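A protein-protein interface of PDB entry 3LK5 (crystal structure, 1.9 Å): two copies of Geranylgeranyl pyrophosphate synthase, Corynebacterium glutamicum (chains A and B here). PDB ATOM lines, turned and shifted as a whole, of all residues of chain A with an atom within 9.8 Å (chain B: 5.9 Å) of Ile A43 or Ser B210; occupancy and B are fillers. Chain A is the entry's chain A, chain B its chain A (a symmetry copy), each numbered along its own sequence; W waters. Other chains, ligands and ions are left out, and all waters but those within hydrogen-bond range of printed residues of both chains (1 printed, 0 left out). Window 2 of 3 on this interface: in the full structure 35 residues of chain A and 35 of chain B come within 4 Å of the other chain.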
ATOM      1  N   GLN A  36     -12.629 -15.436   7.554  1.00  0.00           N
ATOM      2  CA  GLN A  36     -12.019 -14.879   6.329  1.00  0.00           C
ATOM      3  C   GLN A  36     -10.817 -13.982   6.619  1.00  0.00           C
ATOM      4  O   GLN A  36     -10.116 -13.596   5.694  1.00  0.00           O
ATOM      5  CB  GLN A  36     -13.033 -14.026   5.538  1.00  0.00           C
ATOM      6  CG  GLN A  36     -14.490 -14.624   5.349  1.00  0.00           C
ATOM      7  CD  GLN A  36     -14.526 -16.068   4.849  1.00  0.00           C
ATOM      8  OE1 GLN A  36     -13.970 -16.370   3.794  1.00  0.00           O
ATOM      9  NE2 GLN A  36     -15.152 -16.992   5.648  1.00  0.00           N
ATOM     10  N   GLU A  37     -10.597 -13.627   7.884  1.00  0.00           N
ATOM     11  CA  GLU A  37      -9.578 -12.631   8.197  1.00  0.00           C
ATOM     12  C   GLU A  37      -8.164 -12.965   7.728  1.00  0.00           C
ATOM     13  O   GLU A  37      -7.516 -12.110   7.148  1.00  0.00           O
ATOM     14  CB  GLU A  37      -9.596 -12.305   9.677  1.00  0.00           C
ATOM     15  CG  GLU A  37     -10.847 -11.546  10.067  1.00  0.00           C
ATOM     16  CD  GLU A  37     -10.904 -11.311  11.568  1.00  0.00           C
ATOM     17  OE1 GLU A  37      -9.971 -11.732  12.284  1.00  0.00           O
ATOM     18  OE2 GLU A  37     -11.861 -10.701  12.011  1.00  0.00           O
ATOM     19  N   LEU A  38      -7.696 -14.180   7.978  1.00  0.00           N
ATOM     20  CA  LEU A  38      -6.348 -14.573   7.565  1.00  0.00           C
ATOM     21  C   LEU A  38      -6.132 -14.483   6.061  1.00  0.00           C
ATOM     22  O   LEU A  38      -5.110 -13.968   5.605  1.00  0.00           O
ATOM     23  CB  LEU A  38      -6.002 -15.979   8.078  1.00  0.00           C
ATOM     24  CG  LEU A  38      -5.543 -16.045   9.548  1.00  0.00           C
ATOM     25  CD1 LEU A  38      -5.523 -17.478  10.038  1.00  0.00           C
ATOM     26  CD2 LEU A  38      -4.139 -15.415   9.747  1.00  0.00           C
ATOM     27  N   THR A  39      -7.079 -15.017   5.292  1.00  0.00           N
ATOM     28  CA  THR A  39      -6.981 -14.986   3.823  1.00  0.00           C
ATOM     29  C   THR A  39      -6.937 -13.567   3.307  1.00  0.00           C
ATOM     30  O   THR A  39      -6.160 -13.246   2.416  1.00  0.00           O
ATOM     31  CB  THR A  39      -8.204 -15.674   3.173  1.00  0.00           C
ATOM     32  OG1 THR A  39      -8.223 -17.040   3.609  1.00  0.00           O
ATOM     33  CG2 THR A  39      -8.084 -15.592   1.620  1.00  0.00           C
ATOM     34  N   ILE A  40      -7.784 -12.714   3.862  1.00  0.00           N
ATOM     35  CA  ILE A  40      -7.833 -11.323   3.439  1.00  0.00           C
ATOM     36  C   ILE A  40      -6.500 -10.610   3.799  1.00  0.00           C
ATOM     37  O   ILE A  40      -5.952  -9.837   2.989  1.00  0.00           O
ATOM     38  CB  ILE A  40      -9.067 -10.608   4.059  1.00  0.00           C
ATOM     39  CG1 ILE A  40     -10.412 -11.161   3.460  1.00  0.00           C
ATOM     40  CG2 ILE A  40      -9.021  -9.083   3.867  1.00  0.00           C
ATOM     41  CD1 ILE A  40     -10.513 -10.956   1.920  1.00  0.00           C
ATOM     42  N   ALA A  41      -5.994 -10.885   5.002  1.00  0.00           N
ATOM     43  CA  ALA A  41      -4.717 -10.321   5.470  1.00  0.00           C
ATOM     44  C   ALA A  41      -3.520 -10.757   4.610  1.00  0.00           C
ATOM     45  O   ALA A  41      -2.607  -9.937   4.356  1.00  0.00           O
ATOM     46  CB  ALA A  41      -4.502 -10.662   6.956  1.00  0.00           C
ATOM     47  N   ASP A  42      -3.512 -12.013   4.159  1.00  0.00           N
ATOM     48  CA  ASP A  42      -2.458 -12.520   3.215  1.00  0.00           C
ATOM     49  C   ASP A  42      -2.417 -11.697   1.908  1.00  0.00           C
ATOM     50  O   ASP A  42      -1.377 -11.660   1.220  1.00  0.00           O
ATOM     51  CB  ASP A  42      -2.655 -14.008   2.870  1.00  0.00           C
ATOM     52  CG  ASP A  42      -2.329 -14.981   4.031  1.00  0.00           C
ATOM     53  OD1 ASP A  42      -1.591 -14.620   4.969  1.00  0.00           O
ATOM     54  OD2 ASP A  42      -2.808 -16.156   3.993  1.00  0.00           O
ATOM     55  N   ILE A  43      -3.531 -11.039   1.562  1.00  0.00           N
ATOM     56  CA  ILE A  43      -3.623 -10.189   0.353  1.00  0.00           C
ATOM     57  C   ILE A  43      -3.110  -8.772   0.622  1.00  0.00           C
ATOM     58  O   ILE A  43      -2.281  -8.236  -0.138  1.00  0.00           O
ATOM     59  CB  ILE A  43      -5.050 -10.119  -0.278  1.00  0.00           C
ATOM     60  CG1 ILE A  43      -5.556 -11.518  -0.643  1.00  0.00           C
ATOM     61  CG2 ILE A  43      -5.026  -9.184  -1.526  1.00  0.00           C
ATOM     62  CD1 ILE A  43      -7.004 -11.547  -1.090  1.00  0.00           C
ATOM     63  N   GLY A  44      -3.556  -8.170   1.710  1.00  0.00           N
ATOM     64  CA  GLY A  44      -2.946  -6.903   2.130  1.00  0.00           C
ATOM     65  C   GLY A  44      -3.805  -6.097   3.078  1.00  0.00           C
ATOM     66  O   GLY A  44      -5.011  -6.279   3.136  1.00  0.00           O
ATOM     67  N   ALA A  45      -3.184  -5.160   3.801  1.00  0.00           N
ATOM     68  CA  ALA A  45      -3.896  -4.343   4.781  1.00  0.00           C
ATOM     69  C   ALA A  45      -5.058  -3.520   4.212  1.00  0.00           C
ATOM     70  O   ALA A  45      -6.119  -3.450   4.841  1.00  0.00           O
ATOM     71  CB  ALA A  45      -2.890  -3.429   5.571  1.00  0.00           C
ATOM     72  N   PRO A  46      -4.910  -2.931   3.001  1.00  0.00           N
ATOM     73  CA  PRO A  46      -6.064  -2.149   2.497  1.00  0.00           C
ATOM     74  C   PRO A  46      -7.286  -3.020   2.213  1.00  0.00           C
ATOM     75  O   PRO A  46      -8.419  -2.529   2.232  1.00  0.00           O
ATOM     76  CB  PRO A  46      -5.530  -1.552   1.172  1.00  0.00           C
ATOM     77  CG  PRO A  46      -4.051  -1.532   1.356  1.00  0.00           C
ATOM     78  CD  PRO A  46      -3.759  -2.817   2.083  1.00  0.00           C
ATOM     79  N   VAL A  47      -7.054  -4.307   1.939  1.00  0.00           N
ATOM     80  CA  VAL A  47      -8.157  -5.247   1.718  1.00  0.00           C
ATOM     81  C   VAL A  47      -8.812  -5.587   3.075  1.00  0.00           C
ATOM     82  O   VAL A  47     -10.031  -5.657   3.181  1.00  0.00           O
ATOM     83  CB  VAL A  47      -7.693  -6.541   1.014  1.00  0.00           C
ATOM     84  CG1 VAL A  47      -8.896  -7.397   0.560  1.00  0.00           C
ATOM     85  CG2 VAL A  47      -6.856  -6.196  -0.235  1.00  0.00           C
ATOM     86  N   THR A  48      -7.988  -5.804   4.093  1.00  0.00           N
ATOM     87  CA  THR A  48      -8.508  -5.886   5.474  1.00  0.00           C
ATOM     88  C   THR A  48      -9.359  -4.677   5.815  1.00  0.00           C
ATOM     89  O   THR A  48     -10.450  -4.837   6.342  1.00  0.00           O
ATOM     90  CB  THR A  48      -7.379  -6.050   6.469  1.00  0.00           C
ATOM     91  OG1 THR A  48      -6.772  -7.323   6.235  1.00  0.00           O
ATOM     92  CG2 THR A  48      -7.885  -5.949   7.940  1.00  0.00           C
ATOM     93  N   ASP A  49      -8.879  -3.471   5.504  1.00  0.00           N
ATOM     94  CA  ASP A  49      -9.652  -2.225   5.765  1.00  0.00           C
ATOM     95  C   ASP A  49     -10.996  -2.185   5.019  1.00  0.00           C
ATOM     96  O   ASP A  49     -12.043  -1.806   5.590  1.00  0.00           O
ATOM     97  CB  ASP A  49      -8.818  -0.955   5.447  1.00  0.00           C
ATOM     98  CG  ASP A  49      -7.540  -0.852   6.282  1.00  0.00           C
ATOM     99  OD1 ASP A  49      -7.472  -1.508   7.340  1.00  0.00           O
ATOM    100  OD2 ASP A  49      -6.590  -0.120   5.881  1.00  0.00           O
ATOM    101  N   VAL A  51     -12.741  -4.841   3.965  1.00  0.00           N
ATOM    102  CA  VAL A  51     -13.609  -5.907   4.473  1.00  0.00           C
ATOM    103  C   VAL A  51     -14.114  -5.517   5.870  1.00  0.00           C
ATOM    104  O   VAL A  51     -15.223  -5.871   6.235  1.00  0.00           O
ATOM    105  CB  VAL A  51     -12.870  -7.276   4.488  1.00  0.00           C
ATOM    106  CG1 VAL A  51     -13.635  -8.340   5.267  1.00  0.00           C
ATOM    107  CG2 VAL A  51     -12.589  -7.752   3.062  1.00  0.00           C
ATOM    108  N   MET A 154     -17.766  -8.862  -3.185  1.00  0.00           N
ATOM    109  CA  MET A 154     -17.269  -9.759  -2.138  1.00  0.00           C
ATOM    110  C   MET A 154     -18.429 -10.371  -1.333  1.00  0.00           C
ATOM    111  O   MET A 154     -18.414 -11.572  -1.049  1.00  0.00           O
ATOM    112  CB  MET A 154     -16.281  -9.050  -1.208  1.00  0.00           C
ATOM    113  CG  MET A 154     -15.544 -10.010  -0.278  1.00  0.00           C
ATOM    114  SD  MET A 154     -14.177 -11.057  -1.210  1.00  0.00           S
ATOM    115  CE  MET A 154     -12.784  -9.667  -1.222  1.00  0.00           C
ATOM    116  N   TRP A 158     -19.362 -14.314  -1.074  1.00  0.00           N
ATOM    117  CA  TRP A 158     -19.403 -14.930   0.264  1.00  0.00           C
ATOM    118  C   TRP A 158     -20.792 -15.498   0.616  1.00  0.00           C
ATOM    119  O   TRP A 158     -20.876 -16.435   1.405  1.00  0.00           O
ATOM    120  CB  TRP A 158     -18.950 -13.911   1.322  1.00  0.00           C
ATOM    121  CG  TRP A 158     -17.436 -13.775   1.294  1.00  0.00           C
ATOM    122  CD1 TRP A 158     -16.540 -14.535   0.568  1.00  0.00           C
ATOM    123  CD2 TRP A 158     -16.659 -12.861   2.069  1.00  0.00           C
ATOM    124  NE1 TRP A 158     -15.227 -14.088   0.816  1.00  0.00           N
ATOM    125  CE2 TRP A 158     -15.297 -13.082   1.753  1.00  0.00           C
ATOM    126  CE3 TRP A 158     -16.997 -11.841   2.987  1.00  0.00           C
ATOM    127  CZ2 TRP A 158     -14.269 -12.332   2.333  1.00  0.00           C
ATOM    128  CZ3 TRP A 158     -15.973 -11.082   3.556  1.00  0.00           C
ATOM    129  CH2 TRP A 158     -14.628 -11.340   3.232  1.00  0.00           C
ATOM    130  N   THR B 185     -12.378 -15.042  -3.883  1.00  0.00           N
ATOM    131  CA  THR B 185     -11.931 -14.098  -2.842  1.00  0.00           C
ATOM    132  C   THR B 185     -10.639 -13.403  -3.314  1.00  0.00           C
ATOM    133  O   THR B 185     -10.453 -12.192  -3.109  1.00  0.00           O
ATOM    134  CB  THR B 185     -11.772 -14.807  -1.504  1.00  0.00           C
ATOM    135  OG1 THR B 185     -13.099 -15.105  -1.018  1.00  0.00           O
ATOM    136  CG2 THR B 185     -11.060 -13.879  -0.463  1.00  0.00           C
ATOM    137  N   GLU B 186      -9.744 -14.187  -3.927  1.00  0.00           N
ATOM    138  CA  GLU B 186      -8.439 -13.643  -4.369  1.00  0.00           C
ATOM    139  C   GLU B 186      -8.579 -12.566  -5.437  1.00  0.00           C
ATOM    140  O   GLU B 186      -7.930 -11.509  -5.352  1.00  0.00           O
ATOM    141  CB  GLU B 186      -7.516 -14.799  -4.815  1.00  0.00           C
ATOM    142  CG  GLU B 186      -6.965 -15.586  -3.616  1.00  0.00           C
ATOM    143  CD  GLU B 186      -6.511 -17.028  -3.924  1.00  0.00           C
ATOM    144  OE1 GLU B 186      -6.585 -17.519  -5.076  1.00  0.00           O
ATOM    145  OE2 GLU B 186      -6.156 -17.735  -2.959  1.00  0.00           O
ATOM    146  N   GLY B 189     -10.217  -9.487  -3.822  1.00  0.00           N
ATOM    147  CA  GLY B 189      -9.198  -8.933  -2.890  1.00  0.00           C
ATOM    148  C   GLY B 189      -8.060  -8.235  -3.669  1.00  0.00           C
ATOM    149  O   GLY B 189      -7.656  -7.096  -3.328  1.00  0.00           O
ATOM    150  N   GLY B 190      -7.525  -8.913  -4.689  1.00  0.00           N
ATOM    151  CA  GLY B 190      -6.574  -8.261  -5.655  1.00  0.00           C
ATOM    152  C   GLY B 190      -7.052  -6.943  -6.264  1.00  0.00           C
ATOM    153  O   GLY B 190      -6.309  -5.952  -6.295  1.00  0.00           O
ATOM    154  N   LEU B 193      -7.032  -4.177  -3.589  1.00  0.00           N
ATOM    155  CA  LEU B 193      -5.671  -3.669  -3.369  1.00  0.00           C
ATOM    156  C   LEU B 193      -5.228  -2.721  -4.493  1.00  0.00           C
ATOM    157  O   LEU B 193      -4.561  -1.709  -4.231  1.00  0.00           O
ATOM    158  CB  LEU B 193      -4.674  -4.823  -3.212  1.00  0.00           C
ATOM    159  CG  LEU B 193      -3.209  -4.458  -2.955  1.00  0.00           C
ATOM    160  CD1 LEU B 193      -3.076  -3.526  -1.718  1.00  0.00           C
ATOM    161  CD2 LEU B 193      -2.442  -5.726  -2.727  1.00  0.00           C
ATOM    162  N   VAL B 205       6.573  -1.264  -5.065  1.00  0.00           N
ATOM    163  CA  VAL B 205       6.807  -2.402  -5.977  1.00  0.00           C
ATOM    164  C   VAL B 205       6.157  -3.647  -5.367  1.00  0.00           C
ATOM    165  O   VAL B 205       5.467  -4.425  -6.061  1.00  0.00           O
ATOM    166  CB  VAL B 205       8.313  -2.659  -6.196  1.00  0.00           C
ATOM    167  CG1 VAL B 205       8.528  -3.857  -7.122  1.00  0.00           C
ATOM    168  CG2 VAL B 205       8.989  -1.435  -6.822  1.00  0.00           C
ATOM    169  N   GLU B 206       6.350  -3.791  -4.051  1.00  0.00           N
ATOM    170  CA  GLU B 206       5.815  -4.905  -3.257  1.00  0.00           C
ATOM    171  C   GLU B 206       4.309  -5.008  -3.346  1.00  0.00           C
ATOM    172  O   GLU B 206       3.743  -6.115  -3.431  1.00  0.00           O
ATOM    173  CB  GLU B 206       6.153  -4.706  -1.788  1.00  0.00           C
ATOM    174  CG  GLU B 206       6.874  -5.864  -1.159  1.00  0.00           C
ATOM    175  CD  GLU B 206       8.293  -5.976  -1.684  1.00  0.00           C
ATOM    176  OE1 GLU B 206       9.014  -4.944  -1.705  1.00  0.00           O
ATOM    177  OE2 GLU B 206       8.692  -7.096  -2.085  1.00  0.00           O
ATOM    178  N   LEU B 207       3.642  -3.861  -3.291  1.00  0.00           N
ATOM    179  CA  LEU B 207       2.195  -3.892  -3.321  1.00  0.00           C
ATOM    180  C   LEU B 207       1.682  -4.192  -4.716  1.00  0.00           C
ATOM    181  O   LEU B 207       0.687  -4.897  -4.872  1.00  0.00           O
ATOM    182  CB  LEU B 207       1.595  -2.618  -2.756  1.00  0.00           C
ATOM    183  CG  LEU B 207       1.745  -2.533  -1.227  1.00  0.00           C
ATOM    184  CD1 LEU B 207       1.382  -1.131  -0.777  1.00  0.00           C
ATOM    185  CD2 LEU B 207       0.898  -3.584  -0.478  1.00  0.00           C
ATOM    186  N   ALA B 208       2.357  -3.657  -5.733  1.00  0.00           N
ATOM    187  CA  ALA B 208       2.028  -3.989  -7.123  1.00  0.00           C
ATOM    188  C   ALA B 208       2.219  -5.489  -7.357  1.00  0.00           C
ATOM    189  O   ALA B 208       1.372  -6.113  -8.046  1.00  0.00           O
ATOM    190  CB  ALA B 208       2.893  -3.165  -8.120  1.00  0.00           C
ATOM    191  N   ASP B 209       3.287  -6.066  -6.786  1.00  0.00           N
ATOM    192  CA  ASP B 209       3.527  -7.539  -6.814  1.00  0.00           C
ATOM    193  C   ASP B 209       2.332  -8.327  -6.234  1.00  0.00           C
ATOM    194  O   ASP B 209       1.931  -9.361  -6.789  1.00  0.00           O
ATOM    195  CB  ASP B 209       4.768  -7.961  -6.003  1.00  0.00           C
ATOM    196  CG  ASP B 209       6.097  -7.559  -6.657  1.00  0.00           C
ATOM    197  OD1 ASP B 209       6.178  -7.342  -7.895  1.00  0.00           O
ATOM    198  OD2 ASP B 209       7.095  -7.479  -5.894  1.00  0.00           O
ATOM    199  N   SER B 210       1.810  -7.856  -5.098  1.00  0.00           N
ATOM    200  CA  SER B 210       0.651  -8.497  -4.484  1.00  0.00           C
ATOM    201  C   SER B 210      -0.551  -8.466  -5.389  1.00  0.00           C
ATOM    202  O   SER B 210      -1.266  -9.477  -5.516  1.00  0.00           O
ATOM    203  CB  SER B 210       0.308  -7.881  -3.121  1.00  0.00           C
ATOM    204  OG  SER B 210       1.383  -8.105  -2.214  1.00  0.00           O
ATOM    205  N   VAL B 211      -0.792  -7.318  -6.011  1.00  0.00           N
ATOM    206  CA  VAL B 211      -1.883  -7.212  -6.954  1.00  0.00           C
ATOM    207  C   VAL B 211      -1.702  -8.264  -8.074  1.00  0.00           C
ATOM    208  O   VAL B 211      -2.644  -8.989  -8.432  1.00  0.00           O
ATOM    209  CB  VAL B 211      -1.969  -5.819  -7.561  1.00  0.00           C
ATOM    210  CG1 VAL B 211      -2.988  -5.808  -8.686  1.00  0.00           C
ATOM    211  CG2 VAL B 211      -2.321  -4.762  -6.486  1.00  0.00           C
ATOM    212  N   ASN B 212      -0.486  -8.345  -8.628  1.00  0.00           N
ATOM    213  CA  ASN B 212      -0.242  -9.322  -9.697  1.00  0.00           C
ATOM    214  C   ASN B 212      -0.495 -10.786  -9.247  1.00  0.00           C
ATOM    215  O   ASN B 212      -1.087 -11.567 -10.005  1.00  0.00           O
ATOM    216  CB  ASN B 212       1.183  -9.181 -10.261  1.00  0.00           C
ATOM    217  CG  ASN B 212       1.402  -7.889 -11.031  1.00  0.00           C
ATOM    218  OD1 ASN B 212       2.578  -7.485 -11.315  1.00  0.00           O
ATOM    219  ND2 ASN B 212       0.321  -7.235 -11.405  1.00  0.00           N
ATOM    220  N   ARG B 213      -0.065 -11.130  -8.034  1.00  0.00           N
ATOM    221  CA  ARG B 213      -0.204 -12.482  -7.475  1.00  0.00           C
ATOM    222  C   ARG B 213      -1.687 -12.916  -7.379  1.00  0.00           C
ATOM    223  O   ARG B 213      -2.024 -14.086  -7.673  1.00  0.00           O
ATOM    224  CB  ARG B 213       0.407 -12.497  -6.082  1.00  0.00           C
ATOM    225  CG  ARG B 213       0.283 -13.779  -5.330  1.00  0.00           C
ATOM    226  CD  ARG B 213       0.978 -13.673  -3.959  1.00  0.00           C
ATOM    227  NE  ARG B 213       0.601 -14.839  -3.153  1.00  0.00           N
ATOM    228  CZ  ARG B 213       0.691 -14.937  -1.823  1.00  0.00           C
ATOM    229  NH1 ARG B 213       1.140 -13.924  -1.078  1.00  0.00           N
ATOM    230  NH2 ARG B 213       0.295 -16.061  -1.236  1.00  0.00           N
ATOM    231  N   PHE B 214      -2.532 -11.957  -6.963  1.00  0.00           N
ATOM    232  CA  PHE B 214      -3.945 -12.257  -6.595  1.00  0.00           C
ATOM    233  C   PHE B 214      -4.923 -11.865  -7.687  1.00  0.00           C
ATOM    234  O   PHE B 214      -5.733 -12.694  -8.096  1.00  0.00           O
ATOM    235  CB  PHE B 214      -4.306 -11.595  -5.245  1.00  0.00           C
ATOM    236  CG  PHE B 214      -3.608 -12.231  -4.082  1.00  0.00           C
ATOM    237  CD1 PHE B 214      -3.944 -13.539  -3.685  1.00  0.00           C
ATOM    238  CD2 PHE B 214      -2.567 -11.569  -3.425  1.00  0.00           C
ATOM    239  CE1 PHE B 214      -3.276 -14.165  -2.594  1.00  0.00           C
ATOM    240  CE2 PHE B 214      -1.917 -12.150  -2.355  1.00  0.00           C
ATOM    241  CZ  PHE B 214      -2.248 -13.455  -1.941  1.00  0.00           C
ATOM    242  N   LYS B 215      -4.822 -10.630  -8.204  1.00  0.00           N
ATOM    243  CA  LYS B 215      -5.744 -10.190  -9.232  1.00  0.00           C
ATOM    244  C   LYS B 215      -5.490 -10.894 -10.574  1.00  0.00           C
ATOM    245  O   LYS B 215      -6.423 -11.145 -11.323  1.00  0.00           O
ATOM    246  CB  LYS B 215      -5.680  -8.669  -9.404  1.00  0.00           C
ATOM    247  CG  LYS B 215      -6.625  -8.102 -10.468  1.00  0.00           C
ATOM    248  CD  LYS B 215      -6.477  -6.572 -10.632  1.00  0.00           C
ATOM    249  CE  LYS B 215      -6.676  -6.205 -12.102  1.00  0.00           C
ATOM    250  NZ  LYS B 215      -6.928  -4.752 -12.334  1.00  0.00           N
HETATM  251  O   HOH W   1     -12.593 -16.786   1.155  1.00  0.00           O
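The side-chain hydroxyl (OG1) of Thr B185 sits at hydrogen-bond distance from the indole nitrogen (NE1) of Trp A158 (3.0 Å).
The side-chain sulfur (SD) of Met A154 sits close to the indole nitrogen (NE1) of Trp A158 (3.8 Å).
The side-chain hydroxyl (OG) of Ser B210 lies within hydrogen-bond range of the backbone carbonyl oxygen (O) of Glu B206, at 3.3 Å.
Ile A40 touches Thr B185.
Ile A43 touches Gly B189 (CG2 to O, 3.8 Å).
Ile A43 touches Leu B193.
Ile A43 touches Ser B210 (O to CB, 3.97 Å).
Phe B214 touches Ile A43.
CD1 of Leu B193 touches CG of Pro A46, 3.8 Å away.
Val A47 touches Gly B189.
N of Leu B193 touches CG2 of Val A47 (3.9 Å).
CE of Met A154 touches O of Thr B185, 3.9 Å away.
Met A154 touches Gly B189.
Of chain B, only Gly B189 (3.8 Å), Leu B193 (3.6 Å), Ser B210 (3.97 Å) and Phe B214 (3.8 Å) come within 4 Å of Ile A43.
Ser B210 touches one residue of chain A.
Printed residues of chain A within 4 Å of Gly B189: Ile A43, Val A47 and Met A154.
No residue of chain A comes within 4 Å of Ala B208.
No residue of chain A comes within 4 Å of Asp B209.
No residue of chain A comes within 4 Å of Val B211.
Printed residues of chain B within 4 Å of Val A47: Gly B189 and Leu B193.
Of the printed residues of chain A, Phe B214 touches Asp A42 and Ile A43.
Of the printed residues of chain B, Ile A40 touches Thr B185 (3.8 Å).
Of the printed residues of chain A, Leu B193 touches Ile A43, Pro A46 and Val A47.
Of the printed residues of chain B, Trp A158 touches Thr B185.
Val A51 touches none of the printed residues of chain B.
The nearest printed residue of chain B that does not touch Ile A43 is Gly B190 (4.04 Å).
The nearest residue of chain A that does not touch Ser B210 is Asp A42 (5.7 Å).
The nearest printed residue of chain A that does not touch Phe B214 is Thr A39 (5.9 Å).
Of the 17 printed residues of chain A, 7 touch a printed residue of chain B.
Hydrophobic or aromatic side chains of chain A within 4 Å of the printed part of chain B: Ile A40, Ile A43, Pro A46, Val A47, Met A154 and Trp A158.
Hydrophobic or aromatic side chains of chain B within 4 Å of the printed part of chain A: Leu B193 and Phe B214.
Among the printed residues, 12 pairs touch across the chains.
Among the printed residues, no Asp or Glu carboxylate lies within 4 Å of a Lys or Arg side-chain nitrogen of the other chain.
No position is printed for both chains.
Water W1 lies within hydrogen-bond range of the side-chain hydroxyl (OG1) of Thr B185 (2.8 Å) and the side-chain amide oxygen (OE1) of Gln A36 (3.0 Å).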
